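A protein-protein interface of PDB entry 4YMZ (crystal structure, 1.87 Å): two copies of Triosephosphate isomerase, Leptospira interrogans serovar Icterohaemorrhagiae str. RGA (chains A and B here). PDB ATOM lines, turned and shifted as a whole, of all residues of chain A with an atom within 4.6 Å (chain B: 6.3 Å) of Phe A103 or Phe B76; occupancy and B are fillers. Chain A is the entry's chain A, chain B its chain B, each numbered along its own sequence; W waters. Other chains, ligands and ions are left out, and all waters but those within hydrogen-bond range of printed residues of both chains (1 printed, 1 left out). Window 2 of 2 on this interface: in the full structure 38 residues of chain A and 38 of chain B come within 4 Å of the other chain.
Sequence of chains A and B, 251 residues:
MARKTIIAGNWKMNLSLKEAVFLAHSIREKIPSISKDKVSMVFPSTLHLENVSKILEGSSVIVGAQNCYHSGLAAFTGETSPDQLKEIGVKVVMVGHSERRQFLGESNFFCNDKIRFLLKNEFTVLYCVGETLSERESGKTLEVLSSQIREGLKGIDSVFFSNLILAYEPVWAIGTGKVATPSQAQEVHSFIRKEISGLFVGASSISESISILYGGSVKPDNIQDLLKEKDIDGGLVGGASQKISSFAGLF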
ATOM      1  N   LYS A  12     -18.068  13.181  -7.645  1.00  0.00           N
ATOM      2  CA  LYS A  12     -18.532  11.832  -7.375  1.00  0.00           C
ATOM      3  C   LYS A  12     -17.562  10.756  -7.889  1.00  0.00           C
ATOM      4  O   LYS A  12     -16.336  10.823  -7.723  1.00  0.00           O
ATOM      5  CB  LYS A  12     -19.967  11.711  -7.973  1.00  0.00           C
ATOM      6  CG  LYS A  12     -20.891  12.849  -7.561  1.00  0.00           C
ATOM      7  CD  LYS A  12     -22.389  12.559  -7.865  1.00  0.00           C
ATOM      8  CE  LYS A  12     -23.168  13.714  -7.284  1.00  0.00           C
ATOM      9  NZ  LYS A  12     -24.606  13.523  -7.482  1.00  0.00           N
ATOM     10  N   MET A  13     -18.089   9.737  -8.530  1.00  0.00           N
ATOM     11  CA  MET A  13     -17.270   8.716  -9.129  1.00  0.00           C
ATOM     12  C   MET A  13     -17.301   8.817 -10.688  1.00  0.00           C
ATOM     13  O   MET A  13     -17.177   7.822 -11.403  1.00  0.00           O
ATOM     14  CB  MET A  13     -17.753   7.319  -8.605  1.00  0.00           C
ATOM     15  CG  MET A  13     -16.847   6.163  -8.947  1.00  0.00           C
ATOM     16  SD  MET A  13     -17.583   4.604  -8.331  1.00  0.00           S
ATOM     17  CE  MET A  13     -18.849   4.523  -9.605  1.00  0.00           C
ATOM     18  N   GLN A  66     -14.759  12.893  -0.316  1.00  0.00           N
ATOM     19  CA  GLN A  66     -16.173  12.501  -0.472  1.00  0.00           C
ATOM     20  C   GLN A  66     -16.751  11.627   0.652  1.00  0.00           C
ATOM     21  O   GLN A  66     -17.951  11.549   0.822  1.00  0.00           O
ATOM     22  CB  GLN A  66     -16.330  11.799  -1.812  1.00  0.00           C
ATOM     23  CG  GLN A  66     -16.327  12.737  -3.019  1.00  0.00           C
ATOM     24  CD  GLN A  66     -16.375  11.928  -4.308  1.00  0.00           C
ATOM     25  OE1 GLN A  66     -17.002  10.846  -4.368  1.00  0.00           O
ATOM     26  NE2 GLN A  66     -15.823  12.473  -5.360  1.00  0.00           N
ATOM     27  N   GLU A  99     -26.292   9.531  -2.116  1.00  0.00           N
ATOM     28  CA  GLU A  99     -25.831   8.288  -2.713  1.00  0.00           C
ATOM     29  C   GLU A  99     -25.246   7.376  -1.705  1.00  0.00           C
ATOM     30  O   GLU A  99     -25.443   6.145  -1.808  1.00  0.00           O
ATOM     31  CB  GLU A  99     -24.817   8.550  -3.878  1.00  0.00           C
ATOM     32  CG  GLU A  99     -25.518   9.203  -5.070  1.00  0.00           C
ATOM     33  CD  GLU A  99     -24.686  10.177  -5.798  1.00  0.00           C
ATOM     34  OE1 GLU A  99     -23.447  10.233  -5.513  1.00  0.00           O
ATOM     35  OE2 GLU A  99     -25.245  10.931  -6.619  1.00  0.00           O
ATOM     36  N   ARG A 100     -24.599   7.930  -0.679  1.00  0.00           N
ATOM     37  CA  ARG A 100     -24.172   7.033   0.391  1.00  0.00           C
ATOM     38  C   ARG A 100     -25.305   6.565   1.292  1.00  0.00           C
ATOM     39  O   ARG A 100     -25.280   5.377   1.733  1.00  0.00           O
ATOM     40  CB  ARG A 100     -23.100   7.669   1.198  1.00  0.00           C
ATOM     41  CG  ARG A 100     -21.932   8.086   0.273  1.00  0.00           C
ATOM     42  CD  ARG A 100     -20.598   8.171   1.028  1.00  0.00           C
ATOM     43  NE  ARG A 100     -20.224   6.919   1.655  1.00  0.00           N
ATOM     44  CZ  ARG A 100     -19.701   5.899   0.978  1.00  0.00           C
ATOM     45  NH1 ARG A 100     -19.471   6.031  -0.326  1.00  0.00           N
ATOM     46  NH2 ARG A 100     -19.373   4.794   1.589  1.00  0.00           N
ATOM     47  N   ARG A 101     -26.257   7.434   1.577  1.00  0.00           N
ATOM     48  CA  ARG A 101     -27.412   7.006   2.390  1.00  0.00           C
ATOM     49  C   ARG A 101     -28.218   5.914   1.673  1.00  0.00           C
ATOM     50  O   ARG A 101     -28.572   4.937   2.256  1.00  0.00           O
ATOM     51  CB  ARG A 101     -28.307   8.176   2.731  1.00  0.00           C
ATOM     52  CG  ARG A 101     -27.745   9.239   3.650  1.00  0.00           C
ATOM     53  CD  ARG A 101     -28.680  10.413   3.637  1.00  0.00           C
ATOM     54  NE  ARG A 101     -28.243  11.552   4.411  1.00  0.00           N
ATOM     55  CZ  ARG A 101     -28.391  11.679   5.716  1.00  0.00           C
ATOM     56  NH1 ARG A 101     -29.029  10.737   6.421  1.00  0.00           N
ATOM     57  NH2 ARG A 101     -28.046  12.853   6.289  1.00  0.00           N
ATOM     58  N   GLN A 102     -28.451   6.060   0.392  1.00  0.00           N
ATOM     59  CA  GLN A 102     -29.277   5.137  -0.358  1.00  0.00           C
ATOM     60  C   GLN A 102     -28.603   3.910  -0.891  1.00  0.00           C
ATOM     61  O   GLN A 102     -29.196   2.862  -0.940  1.00  0.00           O
ATOM     62  CB  GLN A 102     -29.944   5.852  -1.524  1.00  0.00           C
ATOM     63  CG  GLN A 102     -30.956   6.874  -1.052  1.00  0.00           C
ATOM     64  CD  GLN A 102     -31.834   7.379  -2.186  1.00  0.00           C
ATOM     65  OE1 GLN A 102     -33.035   7.650  -2.013  1.00  0.00           O
ATOM     66  NE2 GLN A 102     -31.251   7.492  -3.350  1.00  0.00           N
ATOM     67  N   PHE A 103     -27.370   4.011  -1.350  1.00  0.00           N
ATOM     68  CA  PHE A 103     -26.731   2.919  -1.978  1.00  0.00           C
ATOM     69  C   PHE A 103     -25.689   2.279  -1.101  1.00  0.00           C
ATOM     70  O   PHE A 103     -25.327   1.146  -1.342  1.00  0.00           O
ATOM     71  CB  PHE A 103     -26.115   3.388  -3.274  1.00  0.00           C
ATOM     72  CG  PHE A 103     -27.107   3.781  -4.289  1.00  0.00           C
ATOM     73  CD1 PHE A 103     -27.793   2.789  -5.018  1.00  0.00           C
ATOM     74  CD2 PHE A 103     -27.321   5.082  -4.578  1.00  0.00           C
ATOM     75  CE1 PHE A 103     -28.725   3.143  -5.989  1.00  0.00           C
ATOM     76  CE2 PHE A 103     -28.282   5.478  -5.516  1.00  0.00           C
ATOM     77  CZ  PHE A 103     -28.955   4.507  -6.259  1.00  0.00           C
ATOM     78  N   LEU A 104     -25.183   2.972  -0.109  1.00  0.00           N
ATOM     79  CA  LEU A 104     -24.250   2.353   0.842  1.00  0.00           C
ATOM     80  C   LEU A 104     -24.833   2.261   2.268  1.00  0.00           C
ATOM     81  O   LEU A 104     -24.148   1.889   3.234  1.00  0.00           O
ATOM     82  CB  LEU A 104     -22.910   3.136   0.824  1.00  0.00           C
ATOM     83  CG  LEU A 104     -22.047   3.048  -0.453  1.00  0.00           C
ATOM     84  CD1 LEU A 104     -21.590   1.636  -0.716  1.00  0.00           C
ATOM     85  CD2 LEU A 104     -22.608   3.655  -1.724  1.00  0.00           C
ATOM     86  N   GLY A 105     -26.125   2.502   2.392  1.00  0.00           N
ATOM     87  CA  GLY A 105     -26.824   2.308   3.694  1.00  0.00           C
ATOM     88  C   GLY A 105     -26.379   3.182   4.905  1.00  0.00           C
ATOM     89  O   GLY A 105     -26.440   2.771   6.036  1.00  0.00           O
ATOM     90  N   TYR B  69     -16.766  -0.275  -5.981  1.00  0.00           N
ATOM     91  CA  TYR B  69     -18.222  -0.327  -6.179  1.00  0.00           C
ATOM     92  C   TYR B  69     -18.539  -0.992  -7.566  1.00  0.00           C
ATOM     93  O   TYR B  69     -17.713  -0.962  -8.426  1.00  0.00           O
ATOM     94  CB  TYR B  69     -18.820   1.015  -6.132  1.00  0.00           C
ATOM     95  CG  TYR B  69     -20.328   0.987  -6.067  1.00  0.00           C
ATOM     96  CD1 TYR B  69     -20.956   0.623  -4.912  1.00  0.00           C
ATOM     97  CD2 TYR B  69     -21.114   1.385  -7.139  1.00  0.00           C
ATOM     98  CE1 TYR B  69     -22.322   0.550  -4.806  1.00  0.00           C
ATOM     99  CE2 TYR B  69     -22.511   1.337  -7.012  1.00  0.00           C
ATOM    100  CZ  TYR B  69     -23.087   0.942  -5.847  1.00  0.00           C
ATOM    101  OH  TYR B  69     -24.444   0.890  -5.659  1.00  0.00           O
ATOM    102  N   SER B  71     -19.790  -0.598 -10.491  1.00  0.00           N
ATOM    103  CA  SER B  71     -20.183   0.336 -11.517  1.00  0.00           C
ATOM    104  C   SER B  71     -18.938   0.947 -12.193  1.00  0.00           C
ATOM    105  O   SER B  71     -17.935   1.272 -11.534  1.00  0.00           O
ATOM    106  CB  SER B  71     -21.076   1.435 -10.921  1.00  0.00           C
ATOM    107  OG  SER B  71     -21.473   2.395 -11.857  1.00  0.00           O
ATOM    108  N   GLY B  72     -19.085   1.163 -13.494  1.00  0.00           N
ATOM    109  CA  GLY B  72     -18.292   2.034 -14.286  1.00  0.00           C
ATOM    110  C   GLY B  72     -18.520   3.455 -13.808  1.00  0.00           C
ATOM    111  O   GLY B  72     -19.309   3.676 -12.906  1.00  0.00           O
ATOM    112  N   LEU B  73     -17.831   4.418 -14.393  1.00  0.00           N
ATOM    113  CA  LEU B  73     -17.892   5.825 -13.931  1.00  0.00           C
ATOM    114  C   LEU B  73     -19.348   6.250 -13.841  1.00  0.00           C
ATOM    115  O   LEU B  73     -20.123   6.037 -14.777  1.00  0.00           O
ATOM    116  CB  LEU B  73     -17.109   6.776 -14.897  1.00  0.00           C
ATOM    117  CG  LEU B  73     -15.617   6.420 -15.093  1.00  0.00           C
ATOM    118  CD1 LEU B  73     -15.006   7.379 -16.098  1.00  0.00           C
ATOM    119  CD2 LEU B  73     -14.885   6.383 -13.711  1.00  0.00           C
ATOM    120  N   ALA B  74     -19.739   6.847 -12.735  1.00  0.00           N
ATOM    121  CA  ALA B  74     -21.120   7.137 -12.457  1.00  0.00           C
ATOM    122  C   ALA B  74     -21.215   7.993 -11.175  1.00  0.00           C
ATOM    123  O   ALA B  74     -20.184   8.244 -10.439  1.00  0.00           O
ATOM    124  CB  ALA B  74     -21.861   5.824 -12.222  1.00  0.00           C
ATOM    125  N   ALA B  75     -22.455   8.295 -10.814  1.00  0.00           N
ATOM    126  CA  ALA B  75     -22.753   9.179  -9.687  1.00  0.00           C
ATOM    127  C   ALA B  75     -22.879   8.387  -8.344  1.00  0.00           C
ATOM    128  O   ALA B  75     -23.998   8.033  -7.856  1.00  0.00           O
ATOM    129  CB  ALA B  75     -23.991   9.986 -10.040  1.00  0.00           C
ATOM    130  N   PHE B  76     -21.720   7.988  -7.782  1.00  0.00           N
ATOM    131  CA  PHE B  76     -21.690   7.244  -6.475  1.00  0.00           C
ATOM    132  C   PHE B  76     -20.676   7.832  -5.546  1.00  0.00           C
ATOM    133  O   PHE B  76     -19.494   7.393  -5.542  1.00  0.00           O
ATOM    134  CB  PHE B  76     -21.461   5.728  -6.644  1.00  0.00           C
ATOM    135  CG  PHE B  76     -22.627   5.019  -7.324  1.00  0.00           C
ATOM    136  CD1 PHE B  76     -23.821   4.718  -6.636  1.00  0.00           C
ATOM    137  CD2 PHE B  76     -22.542   4.735  -8.704  1.00  0.00           C
ATOM    138  CE1 PHE B  76     -24.903   4.124  -7.315  1.00  0.00           C
ATOM    139  CE2 PHE B  76     -23.601   4.162  -9.384  1.00  0.00           C
ATOM    140  CZ  PHE B  76     -24.777   3.835  -8.680  1.00  0.00           C
ATOM    141  N   THR B  77     -21.141   8.925  -4.850  1.00  0.00           N
ATOM    142  CA  THR B  77     -20.272   9.712  -4.059  1.00  0.00           C
ATOM    143  C   THR B  77     -19.518   8.858  -3.046  1.00  0.00           C
ATOM    144  O   THR B  77     -20.154   8.062  -2.337  1.00  0.00           O
ATOM    145  CB  THR B  77     -21.076  10.762  -3.316  1.00  0.00           C
ATOM    146  OG1 THR B  77     -21.560  11.686  -4.283  1.00  0.00           O
ATOM    147  CG2 THR B  77     -20.186  11.509  -2.376  1.00  0.00           C
ATOM    148  N   GLY B  78     -18.211   9.003  -2.942  1.00  0.00           N
ATOM    149  CA  GLY B  78     -17.379   8.238  -1.957  1.00  0.00           C
ATOM    150  C   GLY B  78     -16.858   6.905  -2.445  1.00  0.00           C
ATOM    151  O   GLY B  78     -15.987   6.248  -1.857  1.00  0.00           O
ATOM    152  N   GLU B  79     -17.382   6.447  -3.562  1.00  0.00           N
ATOM    153  CA  GLU B  79     -16.950   5.140  -4.094  1.00  0.00           C
ATOM    154  C   GLU B  79     -15.872   5.229  -5.174  1.00  0.00           C
ATOM    155  O   GLU B  79     -15.765   6.200  -5.907  1.00  0.00           O
ATOM    156  CB  GLU B  79     -18.132   4.336  -4.660  1.00  0.00           C
ATOM    157  CG  GLU B  79     -19.286   4.004  -3.638  1.00  0.00           C
ATOM    158  CD  GLU B  79     -18.688   3.120  -2.541  1.00  0.00           C
ATOM    159  OE1 GLU B  79     -18.289   1.975  -2.868  1.00  0.00           O
ATOM    160  OE2 GLU B  79     -18.579   3.599  -1.402  1.00  0.00           O
ATOM    161  N   THR B  80     -15.144   4.103  -5.333  1.00  0.00           N
ATOM    162  CA  THR B  80     -14.083   3.894  -6.352  1.00  0.00           C
ATOM    163  C   THR B  80     -14.601   2.883  -7.441  1.00  0.00           C
ATOM    164  O   THR B  80     -15.146   1.836  -7.131  1.00  0.00           O
ATOM    165  CB  THR B  80     -12.845   3.279  -5.720  1.00  0.00           C
ATOM    166  OG1 THR B  80     -12.380   4.133  -4.653  1.00  0.00           O
ATOM    167  CG2 THR B  80     -11.706   3.135  -6.781  1.00  0.00           C
ATOM    168  N   PHE B 110     -24.197  -8.203  -1.740  1.00  0.00           N
ATOM    169  CA  PHE B 110     -23.414  -7.033  -2.172  1.00  0.00           C
ATOM    170  C   PHE B 110     -22.071  -7.550  -2.665  1.00  0.00           C
ATOM    171  O   PHE B 110     -21.636  -7.157  -3.702  1.00  0.00           O
ATOM    172  CB  PHE B 110     -23.227  -6.043  -1.035  1.00  0.00           C
ATOM    173  CG  PHE B 110     -22.715  -4.621  -1.443  1.00  0.00           C
ATOM    174  CD1 PHE B 110     -23.108  -4.000  -2.627  1.00  0.00           C
ATOM    175  CD2 PHE B 110     -21.924  -3.887  -0.565  1.00  0.00           C
ATOM    176  CE1 PHE B 110     -22.644  -2.704  -2.955  1.00  0.00           C
ATOM    177  CE2 PHE B 110     -21.475  -2.557  -0.856  1.00  0.00           C
ATOM    178  CZ  PHE B 110     -21.809  -1.971  -2.054  1.00  0.00           C
HETATM  179  O   HOH W   1     -25.680  -0.339  -3.607  1.00  0.00           O
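No position is printed for both chains.
O of Lys A12 is in hydrogen-bond range of NE2 of Gln A66, 2.9 Å away.
OE2 of Glu A99 lies within salt-bridge range of NZ of Lys A12, 2.8 Å away.
N of Gly A105 lies within hydrogen-bond range of O of Arg A100 (3.1 Å).
The backbone carbonyl oxygen of Thr B80 sits at hydrogen-bond distance from the backbone NH of Tyr B69 (2.9 Å).
Phe A103 touches just these residues of chain B: Tyr B69 and Phe B76.
Printed residues of chain B within 4 Å of Leu A104: Glu B79 (3.6 Å) and Phe B110 (3.9 Å).
Of the printed residues of chain A, Ala B74 touches Met A13.
Of chain A, only Met A13, Glu A99 and Phe A103 come within 4 Å of Phe B76.
The nearest residue of chain A that does not touch Phe B76 is Lys A12 (4.1 Å).
The backbone carbonyl oxygen (O) of Met A13 lies within hydrogen-bond range of the backbone NH (N) of Ala B74, at 3.0 Å.
The backbone NH of Gly B78 is in hydrogen-bond range of the side-chain amide oxygen of Gln A66.
The side-chain carboxylate of Glu A99 is in hydrogen-bond range of the side-chain hydroxyl of Thr B77, at 2.7 Å.
The backbone carbonyl oxygen of Thr B77 is in hydrogen-bond range of the guanidinium group of Arg A100, 2.9 Å away.
The guanidinium group (NH1) of Arg A100 is in salt-bridge range of the side-chain carboxylate (OE2) of Glu B79 (2.8 Å).
The side-chain sulfur of Met A13 lies close to the backbone carbonyl oxygen of Glu B79 (3.4 Å).
O of Ala B75 lies close to OE1 of Glu A99 (3.3 Å).
Among the printed residues, pairs that only touch across the chains: Met A13 with Leu B73 (3.3 Å), Met A13 with Gly B72 (3.4 Å), Arg A100 with Gly B78 (3.5 Å), Gln A66 with Thr B77 (3.5 Å), Met A13 with Phe B76 (3.5 Å), Lys A12 with Thr B77 (3.5 Å), Met A13 with Thr B80 (3.6 Å), Glu A99 with Phe B76 (3.6 Å), Leu A104 with Glu B79 (3.6 Å), Lys A12 with Ala B75 (3.7 Å), Phe A103 with Phe B76 (3.8 Å), Phe A103 with Tyr B69 (3.8 Å), Leu A104 with Phe B110 (3.9 Å) and Met A13 with Ser B71 (3.9 Å).
Printed residues of chain A that touch a printed residue of chain B: Lys A12, Met A13, Gln A66, Glu A99, Arg A100, Phe A103 and Leu A104.
Hydrophobic or aromatic side chains of chain A within 4 Å of the printed part of chain B: Met A13, Phe A103 and Leu A104.
Of the 12 printed residues of chain B, 12 touch a printed residue of chain A.
Hydrophobic or aromatic side chains of chain B within 4 Å of the printed part of chain A: Tyr B69, Leu B73, Ala B75, Phe B76 and Phe B110.
Among the printed residues, Asp or Glu carboxylates within 4 Å of a Lys or Arg side-chain nitrogen of the other chain: Arg A100 with Glu B79 (2.8 Å).
Water W1 bridges the side-chain hydroxyl of Tyr B69 (2.7 Å) and the backbone carbonyl oxygen of Phe A103 (2.7 Å).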
